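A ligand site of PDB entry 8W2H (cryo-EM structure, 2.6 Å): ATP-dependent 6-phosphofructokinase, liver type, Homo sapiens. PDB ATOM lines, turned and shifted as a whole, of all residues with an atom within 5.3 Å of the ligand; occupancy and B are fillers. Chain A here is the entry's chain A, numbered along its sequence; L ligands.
The backbone carbonyl oxygen (O) of Gly 224 sits close to an oxygen (O1) of the ligand (3.4 Å). Thr 193 touches the ligand (O to C6, 3.7 Å). Thr 194 touches the ligand (CG2 to N3, 3.4 Å). NE2 of Gln 197 touches C3 of the ligand, 3.3 Å away. Ala 456 touches the ligand (CA to O3, 3.7 Å).
NH2 of Arg 461 is in hydrogen-bond range of O11 of the ligand, at 2.8 Å. OG of Ser 255 is in hydrogen-bond range of O5 of the ligand, 3.4 Å away. The backbone carbonyl oxygen (O) of Gly 460 lies within hydrogen-bond range of a nitrogen (N3) of the ligand, 3.4 Å away. The guanidinium group (NH2) of Arg 423 lies within salt-bridge range of an oxygen (O2) of the ligand (3.3 Å). NH1 of Arg 419 lies within salt-bridge range of O3 of the ligand (3.1 Å). N of Gly 457 sits at hydrogen-bond distance from O3 of the ligand, 2.8 Å away.
O of Gly 457 is in hydrogen-bond range of NE of Arg 461, at 2.7 Å. N of Ser 255 is in hydrogen-bond range of O of Thr 250 (3.2 Å). The side-chain amide oxygen (OE1) of Gln 197 lies within hydrogen-bond range of the backbone NH (N) of Leu 257, 3.3 Å away. O of Leu 388 lies within hydrogen-bond range of NH1 of Arg 423, at 3.2 Å. The backbone carbonyl oxygen (O) of Leu 257 sits at hydrogen-bond distance from the side-chain hydroxyl (OG) of Ser 255. O of Ala 456 sits at hydrogen-bond distance from NH2 of Arg 461 (3.1 Å).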
ATOM      1  N   THR A 193     -12.232  -5.232  22.652  1.00  0.00           N
ATOM      2  CA  THR A 193     -12.909  -6.510  22.887  1.00  0.00           C
ATOM      3  C   THR A 193     -12.280  -7.299  24.031  1.00  0.00           C
ATOM      4  O   THR A 193     -13.007  -7.979  24.772  1.00  0.00           O
ATOM      5  CB  THR A 193     -12.919  -7.351  21.610  1.00  0.00           C
ATOM      6  OG1 THR A 193     -11.567  -7.592  21.179  1.00  0.00           O
ATOM      7  CG2 THR A 193     -13.691  -6.656  20.492  1.00  0.00           C
ATOM      8  N   THR A 194     -10.955  -7.258  24.197  1.00  0.00           N
ATOM      9  CA  THR A 194     -10.318  -7.995  25.281  1.00  0.00           C
ATOM     10  C   THR A 194     -10.542  -7.349  26.650  1.00  0.00           C
ATOM     11  O   THR A 194     -10.164  -7.942  27.666  1.00  0.00           O
ATOM     12  CB  THR A 194      -8.816  -8.144  25.025  1.00  0.00           C
ATOM     13  OG1 THR A 194      -8.175  -6.862  25.093  1.00  0.00           O
ATOM     14  CG2 THR A 194      -8.564  -8.767  23.650  1.00  0.00           C
ATOM     15  N   THR A 195     -11.124  -6.158  26.700  1.00  0.00           N
ATOM     16  CA  THR A 195     -11.487  -5.508  27.955  1.00  0.00           C
ATOM     17  C   THR A 195     -12.688  -6.196  28.584  1.00  0.00           C
ATOM     18  O   THR A 195     -13.586  -6.677  27.888  1.00  0.00           O
ATOM     19  CB  THR A 195     -11.779  -4.023  27.674  1.00  0.00           C
ATOM     20  OG1 THR A 195     -10.565  -3.346  27.306  1.00  0.00           O
ATOM     21  CG2 THR A 195     -12.414  -3.300  28.859  1.00  0.00           C
ATOM     22  N   GLN A 197     -16.006  -6.069  29.619  1.00  0.00           N
ATOM     23  CA  GLN A 197     -17.030  -5.135  29.149  1.00  0.00           C
ATOM     24  C   GLN A 197     -17.951  -4.725  30.306  1.00  0.00           C
ATOM     25  O   GLN A 197     -18.565  -5.593  30.947  1.00  0.00           O
ATOM     26  CB  GLN A 197     -17.825  -5.767  28.015  1.00  0.00           C
ATOM     27  CG  GLN A 197     -16.966  -6.134  26.792  1.00  0.00           C
ATOM     28  CD  GLN A 197     -17.753  -6.875  25.722  1.00  0.00           C
ATOM     29  OE1 GLN A 197     -18.981  -6.868  25.709  1.00  0.00           O
ATOM     30  NE2 GLN A 197     -17.028  -7.528  24.815  1.00  0.00           N
ATOM     31  N   SER A 223     -12.902  -9.300  13.431  1.00  0.00           N
ATOM     32  CA  SER A 223     -13.421  -8.816  14.710  1.00  0.00           C
ATOM     33  C   SER A 223     -14.841  -9.274  14.999  1.00  0.00           C
ATOM     34  O   SER A 223     -15.330  -9.042  16.113  1.00  0.00           O
ATOM     35  CB  SER A 223     -13.374  -7.283  14.745  1.00  0.00           C
ATOM     36  OG  SER A 223     -14.094  -6.728  13.657  1.00  0.00           O
ATOM     37  N   GLY A 224     -15.527  -9.907  14.044  1.00  0.00           N
ATOM     38  CA  GLY A 224     -16.924 -10.252  14.217  1.00  0.00           C
ATOM     39  C   GLY A 224     -17.791  -9.018  14.348  1.00  0.00           C
ATOM     40  O   GLY A 224     -18.591  -8.903  15.285  1.00  0.00           O
ATOM     41  N   ASP A 226     -20.656  -6.277  14.038  1.00  0.00           N
ATOM     42  CA  ASP A 226     -22.111  -6.386  13.930  1.00  0.00           C
ATOM     43  C   ASP A 226     -22.613  -5.877  12.582  1.00  0.00           C
ATOM     44  O   ASP A 226     -23.580  -6.419  12.050  1.00  0.00           O
ATOM     45  CB  ASP A 226     -22.782  -5.627  15.074  1.00  0.00           C
ATOM     46  CG  ASP A 226     -22.327  -6.118  16.432  1.00  0.00           C
ATOM     47  OD1 ASP A 226     -21.207  -5.761  16.851  1.00  0.00           O
ATOM     48  OD2 ASP A 226     -23.081  -6.866  17.082  1.00  0.00           O
ATOM     49  N   THR A 250     -28.907  -7.414  19.717  1.00  0.00           N
ATOM     50  CA  THR A 250     -27.587  -7.640  20.287  1.00  0.00           C
ATOM     51  C   THR A 250     -27.565  -7.262  21.766  1.00  0.00           C
ATOM     52  O   THR A 250     -26.986  -7.983  22.597  1.00  0.00           O
ATOM     53  CB  THR A 250     -26.534  -6.841  19.513  1.00  0.00           C
ATOM     54  OG1 THR A 250     -26.686  -7.089  18.109  1.00  0.00           O
ATOM     55  CG2 THR A 250     -25.119  -7.224  19.928  1.00  0.00           C
ATOM     56  N   SER A 255     -25.063  -8.936  24.903  1.00  0.00           N
ATOM     57  CA  SER A 255     -23.773  -8.558  24.335  1.00  0.00           C
ATOM     58  C   SER A 255     -23.566  -7.068  24.575  1.00  0.00           C
ATOM     59  O   SER A 255     -24.247  -6.229  23.983  1.00  0.00           O
ATOM     60  CB  SER A 255     -23.759  -8.891  22.847  1.00  0.00           C
ATOM     61  OG  SER A 255     -22.544  -8.494  22.226  1.00  0.00           O
ATOM     62  N   LEU A 257     -21.090  -5.019  23.888  1.00  0.00           N
ATOM     63  CA  LEU A 257     -20.313  -4.255  22.916  1.00  0.00           C
ATOM     64  C   LEU A 257     -20.824  -4.524  21.512  1.00  0.00           C
ATOM     65  O   LEU A 257     -21.018  -5.688  21.133  1.00  0.00           O
ATOM     66  CB  LEU A 257     -18.817  -4.619  23.021  1.00  0.00           C
ATOM     67  CG  LEU A 257     -17.831  -4.025  22.006  1.00  0.00           C
ATOM     68  CD1 LEU A 257     -17.733  -2.509  22.150  1.00  0.00           C
ATOM     69  CD2 LEU A 257     -16.467  -4.684  22.185  1.00  0.00           C
ATOM     70  N   ILE A 259     -19.759  -3.555  17.436  1.00  0.00           N
ATOM     71  CA  ILE A 259     -18.676  -3.096  16.559  1.00  0.00           C
ATOM     72  C   ILE A 259     -19.301  -2.765  15.207  1.00  0.00           C
ATOM     73  O   ILE A 259     -19.953  -3.611  14.600  1.00  0.00           O
ATOM     74  CB  ILE A 259     -17.571  -4.167  16.416  1.00  0.00           C
ATOM     75  CG1 ILE A 259     -16.849  -4.400  17.751  1.00  0.00           C
ATOM     76  CG2 ILE A 259     -16.539  -3.772  15.319  1.00  0.00           C
ATOM     77  CD1 ILE A 259     -16.070  -5.712  17.817  1.00  0.00           C
ATOM     78  N   LEU A 388     -21.900 -15.510   9.302  1.00  0.00           N
ATOM     79  CA  LEU A 388     -21.470 -15.663  10.684  1.00  0.00           C
ATOM     80  C   LEU A 388     -21.936 -14.533  11.582  1.00  0.00           C
ATOM     81  O   LEU A 388     -22.000 -14.722  12.803  1.00  0.00           O
ATOM     82  CB  LEU A 388     -19.948 -15.761  10.744  1.00  0.00           C
ATOM     83  CG  LEU A 388     -19.304 -16.868   9.904  1.00  0.00           C
ATOM     84  CD1 LEU A 388     -17.848 -16.586   9.633  1.00  0.00           C
ATOM     85  CD2 LEU A 388     -19.444 -18.192  10.597  1.00  0.00           C
ATOM     86  N   ALA A 389     -22.269 -13.364  11.022  1.00  0.00           N
ATOM     87  CA  ALA A 389     -22.646 -12.211  11.822  1.00  0.00           C
ATOM     88  C   ALA A 389     -23.938 -12.470  12.584  1.00  0.00           C
ATOM     89  O   ALA A 389     -23.978 -12.367  13.819  1.00  0.00           O
ATOM     90  CB  ALA A 389     -22.774 -10.971  10.934  1.00  0.00           C
ATOM     91  N   ARG A 419     -15.662 -21.720  15.828  1.00  0.00           N
ATOM     92  CA  ARG A 419     -16.797 -20.789  15.734  1.00  0.00           C
ATOM     93  C   ARG A 419     -17.470 -20.899  14.376  1.00  0.00           C
ATOM     94  O   ARG A 419     -18.699 -21.059  14.291  1.00  0.00           O
ATOM     95  CB  ARG A 419     -16.313 -19.354  15.978  1.00  0.00           C
ATOM     96  CG  ARG A 419     -17.437 -18.361  16.243  1.00  0.00           C
ATOM     97  CD  ARG A 419     -17.050 -16.912  16.062  1.00  0.00           C
ATOM     98  NE  ARG A 419     -17.021 -16.539  14.651  1.00  0.00           N
ATOM     99  CZ  ARG A 419     -17.379 -15.373  14.133  1.00  0.00           C
ATOM    100  NH1 ARG A 419     -17.850 -14.379  14.878  1.00  0.00           N
ATOM    101  NH2 ARG A 419     -17.265 -15.177  12.826  1.00  0.00           N
ATOM    102  N   ARG A 423     -21.357 -22.305  13.513  1.00  0.00           N
ATOM    103  CA  ARG A 423     -22.363 -21.495  12.836  1.00  0.00           C
ATOM    104  C   ARG A 423     -22.749 -22.100  11.488  1.00  0.00           C
ATOM    105  O   ARG A 423     -23.942 -22.182  11.152  1.00  0.00           O
ATOM    106  CB  ARG A 423     -21.844 -20.065  12.625  1.00  0.00           C
ATOM    107  CG  ARG A 423     -22.072 -19.126  13.785  1.00  0.00           C
ATOM    108  CD  ARG A 423     -21.169 -19.320  14.961  1.00  0.00           C
ATOM    109  NE  ARG A 423     -21.567 -18.400  16.021  1.00  0.00           N
ATOM    110  CZ  ARG A 423     -21.292 -17.094  16.041  1.00  0.00           C
ATOM    111  NH1 ARG A 423     -20.591 -16.512  15.081  1.00  0.00           N
ATOM    112  NH2 ARG A 423     -21.746 -16.367  17.053  1.00  0.00           N
ATOM    113  N   VAL A 455     -20.448 -20.107  20.869  1.00  0.00           N
ATOM    114  CA  VAL A 455     -19.136 -19.750  20.336  1.00  0.00           C
ATOM    115  C   VAL A 455     -18.983 -18.231  20.187  1.00  0.00           C
ATOM    116  O   VAL A 455     -18.075 -17.763  19.499  1.00  0.00           O
ATOM    117  CB  VAL A 455     -18.857 -20.473  19.004  1.00  0.00           C
ATOM    118  CG1 VAL A 455     -18.743 -21.959  19.239  1.00  0.00           C
ATOM    119  CG2 VAL A 455     -19.933 -20.196  17.954  1.00  0.00           C
ATOM    120  N   ALA A 456     -19.832 -17.447  20.848  1.00  0.00           N
ATOM    121  CA  ALA A 456     -19.819 -16.000  20.706  1.00  0.00           C
ATOM    122  C   ALA A 456     -18.514 -15.402  21.229  1.00  0.00           C
ATOM    123  O   ALA A 456     -18.092 -15.700  22.352  1.00  0.00           O
ATOM    124  CB  ALA A 456     -21.022 -15.402  21.437  1.00  0.00           C
ATOM    125  N   GLY A 457     -17.886 -14.562  20.410  1.00  0.00           N
ATOM    126  CA  GLY A 457     -16.638 -13.917  20.776  1.00  0.00           C
ATOM    127  C   GLY A 457     -15.444 -14.822  20.837  1.00  0.00           C
ATOM    128  O   GLY A 457     -14.466 -14.500  21.531  1.00  0.00           O
ATOM    129  N   TRP A 458     -15.466 -15.946  20.132  1.00  0.00           N
ATOM    130  CA  TRP A 458     -14.358 -16.881  20.118  1.00  0.00           C
ATOM    131  C   TRP A 458     -13.287 -16.557  19.072  1.00  0.00           C
ATOM    132  O   TRP A 458     -12.248 -17.225  19.050  1.00  0.00           O
ATOM    133  CB  TRP A 458     -14.883 -18.311  19.873  1.00  0.00           C
ATOM    134  CG  TRP A 458     -15.495 -18.956  21.077  1.00  0.00           C
ATOM    135  CD1 TRP A 458     -16.058 -18.330  22.157  1.00  0.00           C
ATOM    136  CD2 TRP A 458     -15.604 -20.365  21.341  1.00  0.00           C
ATOM    137  NE1 TRP A 458     -16.504 -19.264  23.062  1.00  0.00           N
ATOM    138  CE2 TRP A 458     -16.231 -20.509  22.587  1.00  0.00           C
ATOM    139  CE3 TRP A 458     -15.213 -21.507  20.629  1.00  0.00           C
ATOM    140  CZ2 TRP A 458     -16.504 -21.763  23.139  1.00  0.00           C
ATOM    141  CZ3 TRP A 458     -15.474 -22.747  21.189  1.00  0.00           C
ATOM    142  CH2 TRP A 458     -16.116 -22.863  22.430  1.00  0.00           C
ATOM    143  N   LEU A 459     -13.520 -15.545  18.220  1.00  0.00           N
ATOM    144  CA  LEU A 459     -12.549 -15.192  17.189  1.00  0.00           C
ATOM    145  C   LEU A 459     -11.196 -14.807  17.781  1.00  0.00           C
ATOM    146  O   LEU A 459     -10.183 -15.474  17.536  1.00  0.00           O
ATOM    147  CB  LEU A 459     -13.093 -14.042  16.331  1.00  0.00           C
ATOM    148  CG  LEU A 459     -13.920 -14.401  15.096  1.00  0.00           C
ATOM    149  CD1 LEU A 459     -14.660 -13.185  14.558  1.00  0.00           C
ATOM    150  CD2 LEU A 459     -13.040 -14.993  14.005  1.00  0.00           C
ATOM    151  N   GLY A 460     -11.162 -13.736  18.569  1.00  0.00           N
ATOM    152  CA  GLY A 460      -9.911 -13.220  19.090  1.00  0.00           C
ATOM    153  C   GLY A 460      -9.300 -13.976  20.249  1.00  0.00           C
ATOM    154  O   GLY A 460      -8.226 -13.587  20.703  1.00  0.00           O
ATOM    155  N   ARG A 461      -9.945 -15.029  20.741  1.00  0.00           N
ATOM    156  CA  ARG A 461      -9.412 -15.788  21.867  1.00  0.00           C
ATOM    157  C   ARG A 461      -8.362 -16.767  21.376  1.00  0.00           C
ATOM    158  O   ARG A 461      -8.649 -17.632  20.550  1.00  0.00           O
ATOM    159  CB  ARG A 461     -10.525 -16.532  22.600  1.00  0.00           C
ATOM    160  CG  ARG A 461     -11.626 -15.629  23.125  1.00  0.00           C
ATOM    161  CD  ARG A 461     -12.702 -16.413  23.853  1.00  0.00           C
ATOM    162  NE  ARG A 461     -13.950 -15.667  23.934  1.00  0.00           N
ATOM    163  CZ  ARG A 461     -14.975 -15.969  24.719  1.00  0.00           C
ATOM    164  NH1 ARG A 461     -14.928 -16.978  25.579  1.00  0.00           N
ATOM    165  NH2 ARG A 461     -16.085 -15.236  24.647  1.00  0.00           N
HETATM  166  P1  LIG L   1     -19.745 -12.901  17.619  1.00  0.00           P
HETATM  167  O1  LIG L   1     -18.964 -11.763  17.154  1.00  0.00           O
HETATM  168  O2  LIG L   1     -20.475 -13.349  16.432  1.00  0.00           O
HETATM  169  O3  LIG L   1     -18.758 -13.947  17.861  1.00  0.00           O
HETATM  170  P2  LIG L   1     -20.437 -11.350  19.971  1.00  0.00           P
HETATM  171  O4  LIG L   1     -21.059 -11.610  21.269  1.00  0.00           O
HETATM  172  O5  LIG L   1     -21.119 -10.130  19.572  1.00  0.00           O
HETATM  173  O6  LIG L   1     -20.717 -12.579  18.912  1.00  0.00           O
HETATM  174  P3  LIG L   1     -18.110 -10.462  21.466  1.00  0.00           P
HETATM  175  O7  LIG L   1     -16.729 -10.909  21.533  1.00  0.00           O
HETATM  176  O8  LIG L   1     -17.934  -9.020  21.325  1.00  0.00           O
HETATM  177  O9  LIG L   1     -18.818 -11.107  20.126  1.00  0.00           O
HETATM  178  O10 LIG L   1     -18.945 -10.830  22.841  1.00  0.00           O
HETATM  179  C1  LIG L   1     -18.787 -12.070  23.481  1.00  0.00           C
HETATM  180  C2  LIG L   1     -17.693 -12.090  24.516  1.00  0.00           C
HETATM  181  O11 LIG L   1     -16.382 -12.570  23.972  1.00  0.00           O
HETATM  182  C3  LIG L   1     -17.385 -10.760  25.113  1.00  0.00           C
HETATM  183  O12 LIG L   1     -18.203 -10.559  26.301  1.00  0.00           O
HETATM  184  C4  LIG L   1     -15.976 -10.766  25.474  1.00  0.00           C
HETATM  185  O13 LIG L   1     -15.843 -10.705  26.921  1.00  0.00           O
HETATM  186  C5  LIG L   1     -15.385 -12.034  24.961  1.00  0.00           C
HETATM  187  N1  LIG L   1     -14.117 -11.846  24.342  1.00  0.00           N
HETATM  188  C6  LIG L   1     -13.947 -11.184  23.139  1.00  0.00           C
HETATM  189  N2  LIG L   1     -12.633 -11.283  22.964  1.00  0.00           N
HETATM  190  C7  LIG L   1     -11.911 -11.946  23.940  1.00  0.00           C
HETATM  191  C8  LIG L   1     -10.627 -12.343  24.313  1.00  0.00           C
HETATM  192  N3  LIG L   1      -9.470 -12.067  23.487  1.00  0.00           N
HETATM  193  N4  LIG L   1     -10.514 -13.012  25.424  1.00  0.00           N
HETATM  194  C9  LIG L   1     -11.486 -13.333  26.215  1.00  0.00           C
HETATM  195  N5  LIG L   1     -12.743 -13.021  26.012  1.00  0.00           N
HETATM  196  C10 LIG L   1     -12.940 -12.341  24.877  1.00  0.00           C
